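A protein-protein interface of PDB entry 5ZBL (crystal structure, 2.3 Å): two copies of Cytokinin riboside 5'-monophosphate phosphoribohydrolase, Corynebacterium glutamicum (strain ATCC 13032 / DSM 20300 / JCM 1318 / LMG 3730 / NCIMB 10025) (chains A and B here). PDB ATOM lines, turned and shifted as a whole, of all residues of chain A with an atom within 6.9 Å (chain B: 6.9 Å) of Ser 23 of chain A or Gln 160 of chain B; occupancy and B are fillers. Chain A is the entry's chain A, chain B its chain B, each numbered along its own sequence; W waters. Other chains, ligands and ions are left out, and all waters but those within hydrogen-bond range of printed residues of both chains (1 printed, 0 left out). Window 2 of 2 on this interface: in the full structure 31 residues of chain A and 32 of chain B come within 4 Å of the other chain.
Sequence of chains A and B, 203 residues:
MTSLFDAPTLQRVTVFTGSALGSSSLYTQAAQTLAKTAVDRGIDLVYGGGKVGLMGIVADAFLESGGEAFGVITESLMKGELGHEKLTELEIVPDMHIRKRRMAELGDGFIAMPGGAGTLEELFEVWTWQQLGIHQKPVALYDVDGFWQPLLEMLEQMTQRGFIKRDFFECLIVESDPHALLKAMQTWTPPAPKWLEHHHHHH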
ATOM      1  N   LEU A  21     -11.485  28.300   0.982  1.00  0.00           N
ATOM      2  CA  LEU A  21     -12.642  28.984   0.410  1.00  0.00           C
ATOM      3  C   LEU A  21     -13.260  28.217  -0.713  1.00  0.00           C
ATOM      4  O   LEU A  21     -14.438  28.403  -1.025  1.00  0.00           O
ATOM      5  CB  LEU A  21     -12.247  30.365  -0.114  1.00  0.00           C
ATOM      6  CG  LEU A  21     -11.786  31.388   0.952  1.00  0.00           C
ATOM      7  CD1 LEU A  21     -11.059  32.539   0.280  1.00  0.00           C
ATOM      8  CD2 LEU A  21     -12.949  31.893   1.801  1.00  0.00           C
ATOM      9  N   GLY A  22     -12.483  27.377  -1.361  1.00  0.00           N
ATOM     10  CA  GLY A  22     -12.958  26.716  -2.569  1.00  0.00           C
ATOM     11  C   GLY A  22     -12.709  27.578  -3.805  1.00  0.00           C
ATOM     12  O   GLY A  22     -12.405  28.757  -3.701  1.00  0.00           O
ATOM     13  N   SER A  23     -12.879  26.972  -4.973  1.00  0.00           N
ATOM     14  CA  SER A  23     -12.436  27.539  -6.234  1.00  0.00           C
ATOM     15  C   SER A  23     -13.465  28.502  -6.843  1.00  0.00           C
ATOM     16  O   SER A  23     -13.225  29.042  -7.917  1.00  0.00           O
ATOM     17  CB  SER A  23     -12.177  26.409  -7.230  1.00  0.00           C
ATOM     18  OG  SER A  23     -13.419  25.915  -7.757  1.00  0.00           O
ATOM     19  N   SER A  24     -14.630  28.666  -6.212  1.00  0.00           N
ATOM     20  CA  SER A  24     -15.612  29.674  -6.649  1.00  0.00           C
ATOM     21  C   SER A  24     -16.155  30.517  -5.466  1.00  0.00           C
ATOM     22  O   SER A  24     -16.183  30.073  -4.309  1.00  0.00           O
ATOM     23  CB  SER A  24     -16.753  28.983  -7.402  1.00  0.00           C
ATOM     24  OG  SER A  24     -18.022  29.515  -7.001  1.00  0.00           O
ATOM     25  N   SER A  25     -16.646  31.707  -5.763  1.00  0.00           N
ATOM     26  CA  SER A  25     -17.219  32.566  -4.721  1.00  0.00           C
ATOM     27  C   SER A  25     -18.600  32.124  -4.254  1.00  0.00           C
ATOM     28  O   SER A  25     -19.134  32.721  -3.342  1.00  0.00           O
ATOM     29  CB  SER A  25     -17.348  33.996  -5.241  1.00  0.00           C
ATOM     30  OG  SER A  25     -18.517  34.086  -6.035  1.00  0.00           O
ATOM     31  N   LEU A  26     -19.212  31.169  -4.960  1.00  0.00           N
ATOM     32  CA  LEU A  26     -20.521  30.656  -4.632  1.00  0.00           C
ATOM     33  C   LEU A  26     -20.577  30.108  -3.219  1.00  0.00           C
ATOM     34  O   LEU A  26     -21.589  30.288  -2.522  1.00  0.00           O
ATOM     35  CB  LEU A  26     -20.918  29.539  -5.608  1.00  0.00           C
ATOM     36  CG  LEU A  26     -22.241  28.802  -5.339  1.00  0.00           C
ATOM     37  CD1 LEU A  26     -23.439  29.758  -5.230  1.00  0.00           C
ATOM     38  CD2 LEU A  26     -22.474  27.779  -6.430  1.00  0.00           C
ATOM     39  N   TYR A  27     -19.491  29.452  -2.801  1.00  0.00           N
ATOM     40  CA  TYR A  27     -19.414  28.779  -1.519  1.00  0.00           C
ATOM     41  C   TYR A  27     -19.472  29.797  -0.380  1.00  0.00           C
ATOM     42  O   TYR A  27     -20.264  29.640   0.572  1.00  0.00           O
ATOM     43  CB  TYR A  27     -18.135  27.919  -1.448  1.00  0.00           C
ATOM     44  CG  TYR A  27     -17.979  26.915  -2.586  1.00  0.00           C
ATOM     45  CD1 TYR A  27     -18.951  25.975  -2.842  1.00  0.00           C
ATOM     46  CD2 TYR A  27     -16.849  26.915  -3.386  1.00  0.00           C
ATOM     47  CE1 TYR A  27     -18.825  25.083  -3.878  1.00  0.00           C
ATOM     48  CE2 TYR A  27     -16.718  26.036  -4.424  1.00  0.00           C
ATOM     49  CZ  TYR A  27     -17.716  25.123  -4.668  1.00  0.00           C
ATOM     50  OH  TYR A  27     -17.584  24.228  -5.694  1.00  0.00           O
ATOM     51  N   GLU B 153     -14.741   9.426  -6.727  1.00  0.00           N
ATOM     52  CA  GLU B 153     -15.509  10.489  -7.373  1.00  0.00           C
ATOM     53  C   GLU B 153     -15.813  11.681  -6.436  1.00  0.00           C
ATOM     54  O   GLU B 153     -15.684  12.849  -6.854  1.00  0.00           O
ATOM     55  CB  GLU B 153     -16.817   9.946  -7.992  1.00  0.00           C
ATOM     56  CG  GLU B 153     -17.583  10.954  -8.889  1.00  0.00           C
ATOM     57  CD  GLU B 153     -16.754  11.502 -10.088  1.00  0.00           C
ATOM     58  OE1 GLU B 153     -16.221  10.678 -10.881  1.00  0.00           O
ATOM     59  OE2 GLU B 153     -16.649  12.751 -10.275  1.00  0.00           O
ATOM     60  N   LEU B 155     -13.968  12.543  -3.860  1.00  0.00           N
ATOM     61  CA  LEU B 155     -12.647  13.118  -3.636  1.00  0.00           C
ATOM     62  C   LEU B 155     -12.071  13.924  -4.808  1.00  0.00           C
ATOM     63  O   LEU B 155     -11.423  14.954  -4.617  1.00  0.00           O
ATOM     64  CB  LEU B 155     -11.668  12.008  -3.244  1.00  0.00           C
ATOM     65  CG  LEU B 155     -11.938  11.437  -1.840  1.00  0.00           C
ATOM     66  CD1 LEU B 155     -11.089  10.198  -1.639  1.00  0.00           C
ATOM     67  CD2 LEU B 155     -11.669  12.466  -0.736  1.00  0.00           C
ATOM     68  N   GLU B 156     -12.292  13.423  -6.006  1.00  0.00           N
ATOM     69  CA  GLU B 156     -11.979  14.145  -7.232  1.00  0.00           C
ATOM     70  C   GLU B 156     -12.827  15.395  -7.345  1.00  0.00           C
ATOM     71  O   GLU B 156     -12.279  16.483  -7.626  1.00  0.00           O
ATOM     72  CB  GLU B 156     -12.155  13.236  -8.433  1.00  0.00           C
ATOM     73  CG  GLU B 156     -11.041  12.186  -8.489  1.00  0.00           C
ATOM     74  CD  GLU B 156     -11.353  11.018  -9.401  1.00  0.00           C
ATOM     75  OE1 GLU B 156     -11.924  11.259 -10.508  1.00  0.00           O
ATOM     76  OE2 GLU B 156     -11.023   9.867  -8.991  1.00  0.00           O
ATOM     77  N   GLN B 157     -14.137  15.281  -7.066  1.00  0.00           N
ATOM     78  CA  GLN B 157     -14.991  16.476  -7.066  1.00  0.00           C
ATOM     79  C   GLN B 157     -14.488  17.473  -6.019  1.00  0.00           C
ATOM     80  O   GLN B 157     -14.313  18.625  -6.337  1.00  0.00           O
ATOM     81  CB  GLN B 157     -16.508  16.173  -6.953  1.00  0.00           C
ATOM     82  CG  GLN B 157     -17.220  16.093  -8.310  1.00  0.00           C
ATOM     83  CD  GLN B 157     -18.732  15.898  -8.208  1.00  0.00           C
ATOM     84  OE1 GLN B 157     -19.269  14.918  -8.752  1.00  0.00           O
ATOM     85  NE2 GLN B 157     -19.431  16.827  -7.525  1.00  0.00           N
ATOM     86  N   MET B 158     -14.163  17.020  -4.806  1.00  0.00           N
ATOM     87  CA  MET B 158     -13.582  17.916  -3.806  1.00  0.00           C
ATOM     88  C   MET B 158     -12.281  18.605  -4.261  1.00  0.00           C
ATOM     89  O   MET B 158     -12.034  19.742  -3.881  1.00  0.00           O
ATOM     90  CB  MET B 158     -13.348  17.181  -2.492  1.00  0.00           C
ATOM     91  CG  MET B 158     -14.639  16.897  -1.723  1.00  0.00           C
ATOM     92  SD  MET B 158     -14.400  15.606  -0.470  1.00  0.00           S
ATOM     93  CE  MET B 158     -13.605  16.464   0.841  1.00  0.00           C
ATOM     94  N   THR B 159     -11.449  17.915  -5.038  1.00  0.00           N
ATOM     95  CA  THR B 159     -10.214  18.512  -5.573  1.00  0.00           C
ATOM     96  C   THR B 159     -10.493  19.598  -6.640  1.00  0.00           C
ATOM     97  O   THR B 159      -9.876  20.667  -6.608  1.00  0.00           O
ATOM     98  CB  THR B 159      -9.294  17.435  -6.190  1.00  0.00           C
ATOM     99  OG1 THR B 159      -9.122  16.395  -5.232  1.00  0.00           O
ATOM    100  CG2 THR B 159      -7.944  18.011  -6.561  1.00  0.00           C
ATOM    101  N   GLN B 160     -11.422  19.318  -7.564  1.00  0.00           N
ATOM    102  CA  GLN B 160     -11.812  20.280  -8.599  1.00  0.00           C
ATOM    103  C   GLN B 160     -12.405  21.556  -7.994  1.00  0.00           C
ATOM    104  O   GLN B 160     -12.198  22.665  -8.518  1.00  0.00           O
ATOM    105  CB  GLN B 160     -12.805  19.666  -9.581  1.00  0.00           C
ATOM    106  CG  GLN B 160     -12.197  18.626 -10.532  1.00  0.00           C
ATOM    107  CD  GLN B 160     -13.245  17.788 -11.304  1.00  0.00           C
ATOM    108  OE1 GLN B 160     -12.912  16.728 -11.850  1.00  0.00           O
ATOM    109  NE2 GLN B 160     -14.507  18.261 -11.354  1.00  0.00           N
ATOM    110  N   ARG B 161     -13.156  21.390  -6.908  1.00  0.00           N
ATOM    111  CA  ARG B 161     -13.787  22.501  -6.196  1.00  0.00           C
ATOM    112  C   ARG B 161     -12.825  23.185  -5.208  1.00  0.00           C
ATOM    113  O   ARG B 161     -13.221  24.120  -4.528  1.00  0.00           O
ATOM    114  CB  ARG B 161     -15.016  22.011  -5.436  1.00  0.00           C
ATOM    115  CG  ARG B 161     -16.075  21.290  -6.255  1.00  0.00           C
ATOM    116  CD  ARG B 161     -17.114  20.714  -5.283  1.00  0.00           C
ATOM    117  NE  ARG B 161     -18.345  20.243  -5.911  1.00  0.00           N
ATOM    118  CZ  ARG B 161     -19.342  21.008  -6.359  1.00  0.00           C
ATOM    119  NH1 ARG B 161     -19.293  22.327  -6.301  1.00  0.00           N
ATOM    120  NH2 ARG B 161     -20.410  20.441  -6.882  1.00  0.00           N
ATOM    121  N   GLY B 162     -11.596  22.693  -5.096  1.00  0.00           N
ATOM    122  CA  GLY B 162     -10.539  23.400  -4.413  1.00  0.00           C
ATOM    123  C   GLY B 162     -10.514  23.151  -2.922  1.00  0.00           C
ATOM    124  O   GLY B 162      -9.852  23.879  -2.185  1.00  0.00           O
ATOM    125  N   PHE B 163     -11.215  22.127  -2.449  1.00  0.00           N
ATOM    126  CA  PHE B 163     -11.212  21.783  -1.018  1.00  0.00           C
ATOM    127  C   PHE B 163     -10.135  20.796  -0.555  1.00  0.00           C
ATOM    128  O   PHE B 163      -9.932  20.630   0.665  1.00  0.00           O
ATOM    129  CB  PHE B 163     -12.604  21.325  -0.615  1.00  0.00           C
ATOM    130  CG  PHE B 163     -13.614  22.442  -0.659  1.00  0.00           C
ATOM    131  CD1 PHE B 163     -13.585  23.440   0.303  1.00  0.00           C
ATOM    132  CD2 PHE B 163     -14.536  22.530  -1.686  1.00  0.00           C
ATOM    133  CE1 PHE B 163     -14.480  24.487   0.279  1.00  0.00           C
ATOM    134  CE2 PHE B 163     -15.430  23.578  -1.751  1.00  0.00           C
ATOM    135  CZ  PHE B 163     -15.416  24.556  -0.739  1.00  0.00           C
ATOM    136  N   ILE B 164      -9.442  20.173  -1.512  1.00  0.00           N
ATOM    137  CA  ILE B 164      -8.356  19.211  -1.272  1.00  0.00           C
ATOM    138  C   ILE B 164      -7.306  19.526  -2.329  1.00  0.00           C
ATOM    139  O   ILE B 164      -7.641  19.873  -3.433  1.00  0.00           O
ATOM    140  CB  ILE B 164      -8.886  17.747  -1.421  1.00  0.00           C
ATOM    141  CG1 ILE B 164      -9.552  17.296  -0.125  1.00  0.00           C
ATOM    142  CG2 ILE B 164      -7.786  16.753  -1.767  1.00  0.00           C
ATOM    143  CD1 ILE B 164     -10.091  15.866  -0.155  1.00  0.00           C
HETATM  144  O   HOH W   1      -9.520  26.701  -2.242  1.00  0.00           O
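No position is printed for both chains.
Water W1 bridges O of Gly 162 of chain B (2.8 Å) and N of Gly 22 of chain A (3.2 Å).
The backbone NH (N) of Phe 163 of chain B lies within hydrogen-bond range of the backbone carbonyl oxygen (O) of Met 158 of chain B.
O of Leu 21 of chain A touches CZ of Phe 163 of chain B, 3.98 Å away. Arg 161 of chain B touches Gly 22 of chain A (O to CA, 3.3 Å). CZ of Phe 163 of chain B touches CA of Gly 22 of chain A, at 3.7 Å. O of Gln 160 of chain B touches OG of Ser 23 of chain A, at 3.6 Å. Tyr 27 of chain A touches Phe 163 of chain B (CD2 to CZ, 3.8 Å).
The backbone NH of Ser 23 of chain A sits at hydrogen-bond distance from the backbone carbonyl oxygen of Arg 161 of chain B, at 2.9 Å. The guanidinium group (NH1) of Arg 161 of chain B lies within hydrogen-bond range of the side-chain hydroxyl (OH) of Tyr 27 of chain A, at 2.6 Å.
Of the printed residues of chain B, Leu 21 of chain A touches Phe 163. Of the printed residues of chain B, Gly 22 of chain A touches Arg 161 and Phe 163. Ser 23 of chain A touches two residues of chain B. Printed residues of chain B within 4 Å of Tyr 27 of chain A: Arg 161 and Phe 163. Gln 157 of chain B touches none of the printed residues of chain A. Of chain A, only Ser 23 comes within 4 Å of Gln 160 of chain B. Of the printed residues of chain A, Arg 161 of chain B touches Gly 22 (3.3 Å), Ser 23 (2.9 Å) and Tyr 27 (2.6 Å). Of the printed residues of chain A, Phe 163 of chain B touches Leu 21 (3.98 Å), Gly 22 (3.7 Å) and Tyr 27 (3.8 Å). The nearest printed residue of chain A that does not touch Phe 163 of chain B is Ser 23 of chain A (5.3 Å).
Hydrophobic or aromatic side chains of chain A that line the printed part of chain B: Tyr 27. Among the printed residues, 7 pairs touch across the chains. Among the printed residues, no Asp or Glu carboxylate lies within 4 Å of a Lys or Arg side-chain nitrogen of the other chain.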
